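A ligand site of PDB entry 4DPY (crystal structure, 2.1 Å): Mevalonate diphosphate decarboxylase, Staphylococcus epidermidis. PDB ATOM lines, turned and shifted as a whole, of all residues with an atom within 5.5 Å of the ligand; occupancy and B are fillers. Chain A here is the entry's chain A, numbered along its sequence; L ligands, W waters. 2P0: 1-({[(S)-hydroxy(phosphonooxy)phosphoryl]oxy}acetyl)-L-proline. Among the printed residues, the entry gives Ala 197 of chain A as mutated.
Ala 19 touches the ligand. Lys 22 touches the ligand. Ile 32 touches the ligand. Ala 197 touches the ligand (CB to OAB, 3.2 Å). Met 201 touches the ligand. Met 248 touches the ligand. OD1 of Asp 288 touches CG of the ligand, 3.2 Å away. Hydrophobic or aromatic side chains within 4 Å of the ligand: Ala 19, Tyr 23, Ile 32, Ala 197, Met 201 and Met 248.
N of Tyr 23 lies close to O of the ligand (3.5 Å). The side-chain hydroxyl (OG) of Ser 112 lies within hydrogen-bond range of an oxygen (OAD) of the ligand. An oxygen (O) of the ligand lies within salt-bridge range of the guanidinium group of Arg 149, 3.0 Å away. NE of Arg 198 is in salt-bridge range of OAF of the ligand, at 2.8 Å. An oxygen (OAH) of the ligand sits at hydrogen-bond distance from the backbone NH (N) of Ser 146 (3.0 Å). The side-chain amino group (NZ) of Lys 26 lies within salt-bridge range of an oxygen (OAF) of the ligand, at 2.6 Å. OAC of the ligand is in hydrogen-bond range of OH of Tyr 23 (2.7 Å). OAH of the ligand is in hydrogen-bond range of OG of Ser 146. OG of Ser 144 lies within hydrogen-bond range of OAD of the ligand, at 2.8 Å. N of Gly 145 lies within hydrogen-bond range of OAC of the ligand, at 2.9 Å.
Water W3 bridges an oxygen (OXT) of the ligand (2.8 Å) and the backbone carbonyl oxygen (O) of Asn 17 (3.4 Å). Water W1 bridges N of Ala 289 and OAB of the ligand. Water W5 lies within hydrogen-bond range of N of Ala 19 (2.8 Å), OD1 of Asp 288 (2.9 Å) and OXT of the ligand (3.1 Å).
The side-chain amino group (NZ) of Lys 22 sits close to the backbone carbonyl oxygen (O) of Met 287 (3.3 Å). The side-chain carboxylate of Asp 288 is in salt-bridge range of the side-chain amino group of Lys 22, at 2.7 Å. OD1 of Asn 17 sits at hydrogen-bond distance from NH2 of Arg 149 (2.9 Å). O of Ala 19 sits at hydrogen-bond distance from NZ of Lys 22 (2.8 Å). The guanidinium group of Arg 198 sits at hydrogen-bond distance from the backbone carbonyl oxygen of Gly 143 (3.4 Å). The guanidinium group (NH1) of Arg 149 is in hydrogen-bond range of the side-chain hydroxyl (OG) of Ser 38, at 2.8 Å. The side-chain hydroxyl (OG) of Ser 112 is in hydrogen-bond range of the side-chain hydroxyl (OG) of Ser 144 (2.9 Å). OH of Tyr 23 lies within hydrogen-bond range of SD of Met 201 (3.6 Å).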
ATOM      1  N   ASN A  17       3.501  29.527 -22.833  1.00  0.00           N
ATOM      2  CA  ASN A  17       2.687  28.433 -23.293  1.00  0.00           C
ATOM      3  C   ASN A  17       1.502  28.284 -22.369  1.00  0.00           C
ATOM      4  O   ASN A  17       1.563  28.672 -21.190  1.00  0.00           O
ATOM      5  CB  ASN A  17       3.481  27.111 -23.377  1.00  0.00           C
ATOM      6  CG  ASN A  17       3.743  26.507 -22.016  1.00  0.00           C
ATOM      7  OD1 ASN A  17       2.899  25.795 -21.469  1.00  0.00           O
ATOM      8  ND2 ASN A  17       4.939  26.752 -21.474  1.00  0.00           N
ATOM      9  N   ALA A  19      -1.162  25.352 -20.964  1.00  0.00           N
ATOM     10  CA  ALA A  19      -1.414  23.928 -20.820  1.00  0.00           C
ATOM     11  C   ALA A  19      -2.857  23.605 -21.174  1.00  0.00           C
ATOM     12  O   ALA A  19      -3.776  24.173 -20.593  1.00  0.00           O
ATOM     13  CB  ALA A  19      -1.116  23.478 -19.391  1.00  0.00           C
ATOM     14  N   ILE A  21      -3.760  20.146 -21.374  1.00  0.00           N
ATOM     15  CA  ILE A  21      -3.910  19.162 -20.334  1.00  0.00           C
ATOM     16  C   ILE A  21      -3.054  19.652 -19.172  1.00  0.00           C
ATOM     17  O   ILE A  21      -1.851  19.807 -19.327  1.00  0.00           O
ATOM     18  CB  ILE A  21      -3.469  17.774 -20.787  1.00  0.00           C
ATOM     19  CG1 ILE A  21      -4.350  17.301 -21.940  1.00  0.00           C
ATOM     20  CG2 ILE A  21      -3.553  16.825 -19.629  1.00  0.00           C
ATOM     21  CD1 ILE A  21      -5.795  16.971 -21.524  1.00  0.00           C
ATOM     22  N   LYS A  22      -3.678  19.886 -18.018  1.00  0.00           N
ATOM     23  CA  LYS A  22      -3.064  20.664 -16.937  1.00  0.00           C
ATOM     24  C   LYS A  22      -1.974  19.962 -16.144  1.00  0.00           C
ATOM     25  O   LYS A  22      -2.098  18.792 -15.775  1.00  0.00           O
ATOM     26  CB  LYS A  22      -4.121  21.157 -15.922  1.00  0.00           C
ATOM     27  CG  LYS A  22      -5.206  22.052 -16.505  1.00  0.00           C
ATOM     28  CD  LYS A  22      -4.616  23.207 -17.296  1.00  0.00           C
ATOM     29  CE  LYS A  22      -5.621  24.329 -17.492  1.00  0.00           C
ATOM     30  NZ  LYS A  22      -5.199  25.311 -18.530  1.00  0.00           N
ATOM     31  N   TYR A  23      -0.905  20.713 -15.876  1.00  0.00           N
ATOM     32  CA  TYR A  23       0.037  20.411 -14.814  1.00  0.00           C
ATOM     33  C   TYR A  23      -0.548  20.981 -13.523  1.00  0.00           C
ATOM     34  O   TYR A  23      -0.873  22.146 -13.471  1.00  0.00           O
ATOM     35  CB  TYR A  23       1.379  21.081 -15.145  1.00  0.00           C
ATOM     36  CG  TYR A  23       2.250  21.434 -13.961  1.00  0.00           C
ATOM     37  CD1 TYR A  23       2.515  20.502 -12.948  1.00  0.00           C
ATOM     38  CD2 TYR A  23       2.850  22.695 -13.875  1.00  0.00           C
ATOM     39  CE1 TYR A  23       3.340  20.834 -11.884  1.00  0.00           C
ATOM     40  CE2 TYR A  23       3.669  23.028 -12.817  1.00  0.00           C
ATOM     41  CZ  TYR A  23       3.915  22.099 -11.829  1.00  0.00           C
ATOM     42  OH  TYR A  23       4.734  22.444 -10.783  1.00  0.00           O
ATOM     43  N   TRP A  24      -0.710  20.152 -12.494  1.00  0.00           N
ATOM     44  CA  TRP A  24      -1.317  20.649 -11.259  1.00  0.00           C
ATOM     45  C   TRP A  24      -0.997  19.731 -10.084  1.00  0.00           C
ATOM     46  O   TRP A  24      -1.620  18.680  -9.908  1.00  0.00           O
ATOM     47  CB  TRP A  24      -2.840  20.813 -11.427  1.00  0.00           C
ATOM     48  CG  TRP A  24      -3.470  21.705 -10.369  1.00  0.00           C
ATOM     49  CD1 TRP A  24      -4.356  21.333  -9.402  1.00  0.00           C
ATOM     50  CD2 TRP A  24      -3.245  23.099 -10.188  1.00  0.00           C
ATOM     51  NE1 TRP A  24      -4.692  22.419  -8.632  1.00  0.00           N
ATOM     52  CE2 TRP A  24      -4.013  23.515  -9.091  1.00  0.00           C
ATOM     53  CE3 TRP A  24      -2.448  24.045 -10.849  1.00  0.00           C
ATOM     54  CZ2 TRP A  24      -4.034  24.835  -8.633  1.00  0.00           C
ATOM     55  CZ3 TRP A  24      -2.454  25.357 -10.391  1.00  0.00           C
ATOM     56  CH2 TRP A  24      -3.239  25.730  -9.299  1.00  0.00           C
ATOM     57  N   LYS A  26       2.656  18.686  -7.518  1.00  0.00           N
ATOM     58  CA  LYS A  26       3.999  18.131  -7.691  1.00  0.00           C
ATOM     59  C   LYS A  26       4.207  16.848  -6.894  1.00  0.00           C
ATOM     60  O   LYS A  26       3.795  16.745  -5.733  1.00  0.00           O
ATOM     61  CB  LYS A  26       5.044  19.153  -7.205  1.00  0.00           C
ATOM     62  CG  LYS A  26       5.141  20.457  -7.984  1.00  0.00           C
ATOM     63  CD  LYS A  26       6.031  21.458  -7.237  1.00  0.00           C
ATOM     64  CE  LYS A  26       6.149  22.787  -7.979  1.00  0.00           C
ATOM     65  NZ  LYS A  26       4.838  23.464  -8.177  1.00  0.00           N
ATOM     66  N   ILE A  32      10.862  20.084  -8.573  1.00  0.00           N
ATOM     67  CA  ILE A  32       9.703  20.317  -9.421  1.00  0.00           C
ATOM     68  C   ILE A  32       9.453  19.125 -10.340  1.00  0.00           C
ATOM     69  O   ILE A  32       9.602  19.199 -11.553  1.00  0.00           O
ATOM     70  CB  ILE A  32       9.852  21.654 -10.186  1.00  0.00           C
ATOM     71  CG1 ILE A  32      10.162  22.774  -9.181  1.00  0.00           C
ATOM     72  CG2 ILE A  32       8.589  21.995 -10.963  1.00  0.00           C
ATOM     73  CD1 ILE A  32      10.216  24.140  -9.791  1.00  0.00           C
ATOM     74  N   SER A  38       1.717  16.798 -18.765  1.00  0.00           N
ATOM     75  CA  SER A  38       0.900  17.916 -19.239  1.00  0.00           C
ATOM     76  C   SER A  38       1.123  18.137 -20.724  1.00  0.00           C
ATOM     77  O   SER A  38       2.083  17.662 -21.287  1.00  0.00           O
ATOM     78  CB  SER A  38       1.188  19.199 -18.440  1.00  0.00           C
ATOM     79  OG  SER A  38       2.565  19.540 -18.454  1.00  0.00           O
ATOM     80  N   SER A 112       6.141  33.087 -15.983  1.00  0.00           N
ATOM     81  CA  SER A 112       7.199  32.228 -15.439  1.00  0.00           C
ATOM     82  C   SER A 112       7.705  31.175 -16.430  1.00  0.00           C
ATOM     83  O   SER A 112       8.892  30.844 -16.425  1.00  0.00           O
ATOM     84  CB  SER A 112       6.784  31.556 -14.112  1.00  0.00           C
ATOM     85  OG  SER A 112       5.863  30.502 -14.328  1.00  0.00           O
ATOM     86  N   GLY A 143      13.394  25.924 -12.564  1.00  0.00           N
ATOM     87  CA  GLY A 143      12.967  27.278 -12.241  1.00  0.00           C
ATOM     88  C   GLY A 143      11.455  27.340 -12.109  1.00  0.00           C
ATOM     89  O   GLY A 143      10.921  27.866 -11.122  1.00  0.00           O
ATOM     90  N   SER A 144      10.767  26.793 -13.104  1.00  0.00           N
ATOM     91  CA  SER A 144       9.313  26.736 -13.110  1.00  0.00           C
ATOM     92  C   SER A 144       8.859  25.547 -13.957  1.00  0.00           C
ATOM     93  O   SER A 144       9.331  25.382 -15.084  1.00  0.00           O
ATOM     94  CB  SER A 144       8.761  28.030 -13.696  1.00  0.00           C
ATOM     95  OG  SER A 144       7.362  28.114 -13.511  1.00  0.00           O
ATOM     96  N   GLY A 145       7.961  24.719 -13.421  1.00  0.00           N
ATOM     97  CA  GLY A 145       7.514  23.516 -14.096  1.00  0.00           C
ATOM     98  C   GLY A 145       7.046  23.770 -15.514  1.00  0.00           C
ATOM     99  O   GLY A 145       7.456  23.086 -16.449  1.00  0.00           O
ATOM    100  N   SER A 146       6.192  24.770 -15.690  1.00  0.00           N
ATOM    101  CA  SER A 146       5.662  25.103 -17.026  1.00  0.00           C
ATOM    102  C   SER A 146       6.727  25.580 -18.007  1.00  0.00           C
ATOM    103  O   SER A 146       6.532  25.493 -19.222  1.00  0.00           O
ATOM    104  CB  SER A 146       4.577  26.170 -16.907  1.00  0.00           C
ATOM    105  OG  SER A 146       5.093  27.332 -16.292  1.00  0.00           O
ATOM    106  N   ALA A 147       7.833  26.101 -17.502  1.00  0.00           N
ATOM    107  CA  ALA A 147       8.925  26.564 -18.352  1.00  0.00           C
ATOM    108  C   ALA A 147       9.553  25.394 -19.108  1.00  0.00           C
ATOM    109  O   ALA A 147      10.153  25.581 -20.178  1.00  0.00           O
ATOM    110  CB  ALA A 147       9.987  27.268 -17.520  1.00  0.00           C
ATOM    111  N   ARG A 149       8.276  23.396 -20.849  1.00  0.00           N
ATOM    112  CA  ARG A 149       7.595  23.239 -22.135  1.00  0.00           C
ATOM    113  C   ARG A 149       7.846  24.374 -23.108  1.00  0.00           C
ATOM    114  O   ARG A 149       7.750  24.193 -24.311  1.00  0.00           O
ATOM    115  CB  ARG A 149       6.072  23.082 -21.945  1.00  0.00           C
ATOM    116  CG  ARG A 149       5.667  21.966 -20.999  1.00  0.00           C
ATOM    117  CD  ARG A 149       4.143  21.832 -20.870  1.00  0.00           C
ATOM    118  NE  ARG A 149       3.493  23.074 -20.473  1.00  0.00           N
ATOM    119  CZ  ARG A 149       2.949  23.287 -19.271  1.00  0.00           C
ATOM    120  NH1 ARG A 149       2.991  22.340 -18.353  1.00  0.00           N
ATOM    121  NH2 ARG A 149       2.379  24.461 -18.997  1.00  0.00           N
ATOM    122  N   TRP A 158       5.116  17.565 -21.374  1.00  0.00           N
ATOM    123  CA  TRP A 158       6.051  17.401 -20.289  1.00  0.00           C
ATOM    124  C   TRP A 158       5.848  15.996 -19.720  1.00  0.00           C
ATOM    125  O   TRP A 158       4.809  15.677 -19.138  1.00  0.00           O
ATOM    126  CB  TRP A 158       5.793  18.491 -19.247  1.00  0.00           C
ATOM    127  CG  TRP A 158       6.616  18.420 -18.024  1.00  0.00           C
ATOM    128  CD1 TRP A 158       7.711  17.620 -17.798  1.00  0.00           C
ATOM    129  CD2 TRP A 158       6.407  19.162 -16.819  1.00  0.00           C
ATOM    130  NE1 TRP A 158       8.197  17.831 -16.529  1.00  0.00           N
ATOM    131  CE2 TRP A 158       7.413  18.775 -15.907  1.00  0.00           C
ATOM    132  CE3 TRP A 158       5.466  20.128 -16.430  1.00  0.00           C
ATOM    133  CZ2 TRP A 158       7.498  19.309 -14.628  1.00  0.00           C
ATOM    134  CZ3 TRP A 158       5.559  20.663 -15.156  1.00  0.00           C
ATOM    135  CH2 TRP A 158       6.562  20.261 -14.270  1.00  0.00           C
ATOM    136  N   ALA A 197       0.073  30.031  -8.154  1.00  0.00           N
ATOM    137  CA  ALA A 197      -0.104  28.679  -8.663  1.00  0.00           C
ATOM    138  C   ALA A 197       0.646  27.623  -7.834  1.00  0.00           C
ATOM    139  O   ALA A 197       0.094  26.567  -7.548  1.00  0.00           O
ATOM    140  CB  ALA A 197       0.286  28.598 -10.138  1.00  0.00           C
ATOM    141  N   ARG A 198       1.888  27.907  -7.453  1.00  0.00           N
ATOM    142  CA  ARG A 198       2.705  26.926  -6.745  1.00  0.00           C
ATOM    143  C   ARG A 198       2.071  26.557  -5.413  1.00  0.00           C
ATOM    144  O   ARG A 198       2.031  25.381  -5.022  1.00  0.00           O
ATOM    145  CB  ARG A 198       4.132  27.465  -6.505  1.00  0.00           C
ATOM    146  CG  ARG A 198       5.036  26.541  -5.680  1.00  0.00           C
ATOM    147  CD  ARG A 198       6.501  26.990  -5.725  1.00  0.00           C
ATOM    148  NE  ARG A 198       7.025  27.027  -7.100  1.00  0.00           N
ATOM    149  CZ  ARG A 198       8.288  27.324  -7.413  1.00  0.00           C
ATOM    150  NH1 ARG A 198       9.154  27.603  -6.464  1.00  0.00           N
ATOM    151  NH2 ARG A 198       8.677  27.345  -8.683  1.00  0.00           N
ATOM    152  N   MET A 201      -1.597  24.794  -6.059  1.00  0.00           N
ATOM    153  CA  MET A 201      -1.548  23.396  -6.472  1.00  0.00           C
ATOM    154  C   MET A 201      -1.007  22.551  -5.336  1.00  0.00           C
ATOM    155  O   MET A 201      -1.364  21.385  -5.205  1.00  0.00           O
ATOM    156  CB  MET A 201      -0.752  23.208  -7.756  1.00  0.00           C
ATOM    157  CG  MET A 201       0.764  23.323  -7.599  1.00  0.00           C
ATOM    158  SD  MET A 201       1.592  22.728  -9.086  1.00  0.00           S
ATOM    159  CE  MET A 201       1.310  24.075 -10.226  1.00  0.00           C
ATOM    160  N   MET A 248      -9.555  20.084 -13.324  1.00  0.00           N
ATOM    161  CA  MET A 248      -8.505  20.746 -12.539  1.00  0.00           C
ATOM    162  C   MET A 248      -9.066  21.736 -11.525  1.00  0.00           C
ATOM    163  O   MET A 248      -8.671  21.743 -10.363  1.00  0.00           O
ATOM    164  CB  MET A 248      -7.525  21.468 -13.462  1.00  0.00           C
ATOM    165  CG  MET A 248      -6.191  21.792 -12.777  1.00  0.00           C
ATOM    166  SD  MET A 248      -5.659  23.468 -13.139  1.00  0.00           S
ATOM    167  CE  MET A 248      -6.684  24.352 -11.961  1.00  0.00           C
ATOM    168  N   MET A 287      -8.856  27.461 -18.316  1.00  0.00           N
ATOM    169  CA  MET A 287      -8.476  28.519 -17.374  1.00  0.00           C
ATOM    170  C   MET A 287      -7.278  28.063 -16.572  1.00  0.00           C
ATOM    171  O   MET A 287      -7.120  26.866 -16.316  1.00  0.00           O
ATOM    172  CB  MET A 287      -9.633  28.848 -16.415  1.00  0.00           C
ATOM    173  CG  MET A 287     -10.803  29.583 -17.064  1.00  0.00           C
ATOM    174  SD  MET A 287     -11.952  28.505 -17.975  1.00  0.00           S
ATOM    175  CE  MET A 287     -12.303  27.201 -16.788  1.00  0.00           C
ATOM    176  N   ASP A 288      -6.448  29.011 -16.143  1.00  0.00           N
ATOM    177  CA  ASP A 288      -5.280  28.678 -15.353  1.00  0.00           C
ATOM    178  C   ASP A 288      -5.417  29.086 -13.886  1.00  0.00           C
ATOM    179  O   ASP A 288      -6.470  28.894 -13.278  1.00  0.00           O
ATOM    180  CB  ASP A 288      -4.033  29.213 -16.023  1.00  0.00           C
ATOM    181  CG  ASP A 288      -3.775  28.524 -17.363  1.00  0.00           C
ATOM    182  OD1 ASP A 288      -3.727  27.278 -17.371  1.00  0.00           O
ATOM    183  OD2 ASP A 288      -3.664  29.194 -18.397  1.00  0.00           O
ATOM    184  N   ALA A 289      -4.352  29.616 -13.296  1.00  0.00           N
ATOM    185  CA  ALA A 289      -4.398  29.986 -11.893  1.00  0.00           C
ATOM    186  C   ALA A 289      -4.910  31.417 -11.738  1.00  0.00           C
ATOM    187  O   ALA A 289      -4.250  32.261 -11.147  1.00  0.00           O
ATOM    188  CB  ALA A 289      -3.020  29.850 -11.247  1.00  0.00           C
HETATM  189  C   2P0 L   1       0.392  24.827 -16.142  1.00  0.00           C
HETATM  190  N   2P0 L   1      -0.647  26.237 -14.390  1.00  0.00           N
HETATM  191  O   2P0 L   1       0.735  23.691 -16.667  1.00  0.00           O
HETATM  192  CA  2P0 L   1      -0.522  24.880 -14.909  1.00  0.00           C
HETATM  193  CB  2P0 L   1      -1.881  24.388 -15.197  1.00  0.00           C
HETATM  194  CD  2P0 L   1      -1.971  26.718 -14.691  1.00  0.00           C
HETATM  195  CG  2P0 L   1      -2.830  25.492 -14.836  1.00  0.00           C
HETATM  196  OAB 2P0 L   1       0.139  28.144 -13.309  1.00  0.00           O
HETATM  197  OAC 2P0 L   1       6.109  24.714 -11.179  1.00  0.00           O
HETATM  198  OAD 2P0 L   1       4.769  28.641 -12.490  1.00  0.00           O
HETATM  199  OAF 2P0 L   1       5.424  25.828  -9.102  1.00  0.00           O
HETATM  200  OAG 2P0 L   1       6.677  27.128 -10.827  1.00  0.00           O
HETATM  201  OAH 2P0 L   1       4.742  26.446 -13.708  1.00  0.00           O
HETATM  202  CAK 2P0 L   1       1.719  26.429 -13.412  1.00  0.00           C
HETATM  203  OAM 2P0 L   1       2.588  27.489 -12.909  1.00  0.00           O
HETATM  204  OAN 2P0 L   1       4.268  26.499 -11.207  1.00  0.00           O
HETATM  205  CAP 2P0 L   1       0.383  27.004 -13.679  1.00  0.00           C
HETATM  206  PAS 2P0 L   1       5.638  26.035 -10.569  1.00  0.00           P
HETATM  207  PAT 2P0 L   1       4.132  27.254 -12.586  1.00  0.00           P
HETATM  208  OXT 2P0 L   1       0.834  25.894 -16.686  1.00  0.00           O
HETATM  209  O   HOH W   1      -1.604  30.442 -14.123  1.00  0.00           O
HETATM  210  O   HOH W   2       2.338  30.230 -13.176  1.00  0.00           O
HETATM  211  O   HOH W   3       1.898  28.215 -17.791  1.00  0.00           O
HETATM  212  O   HOH W   4       5.808  29.642 -10.334  1.00  0.00           O
HETATM  213  O   HOH W   5      -1.156  27.081 -18.707  1.00  0.00           O
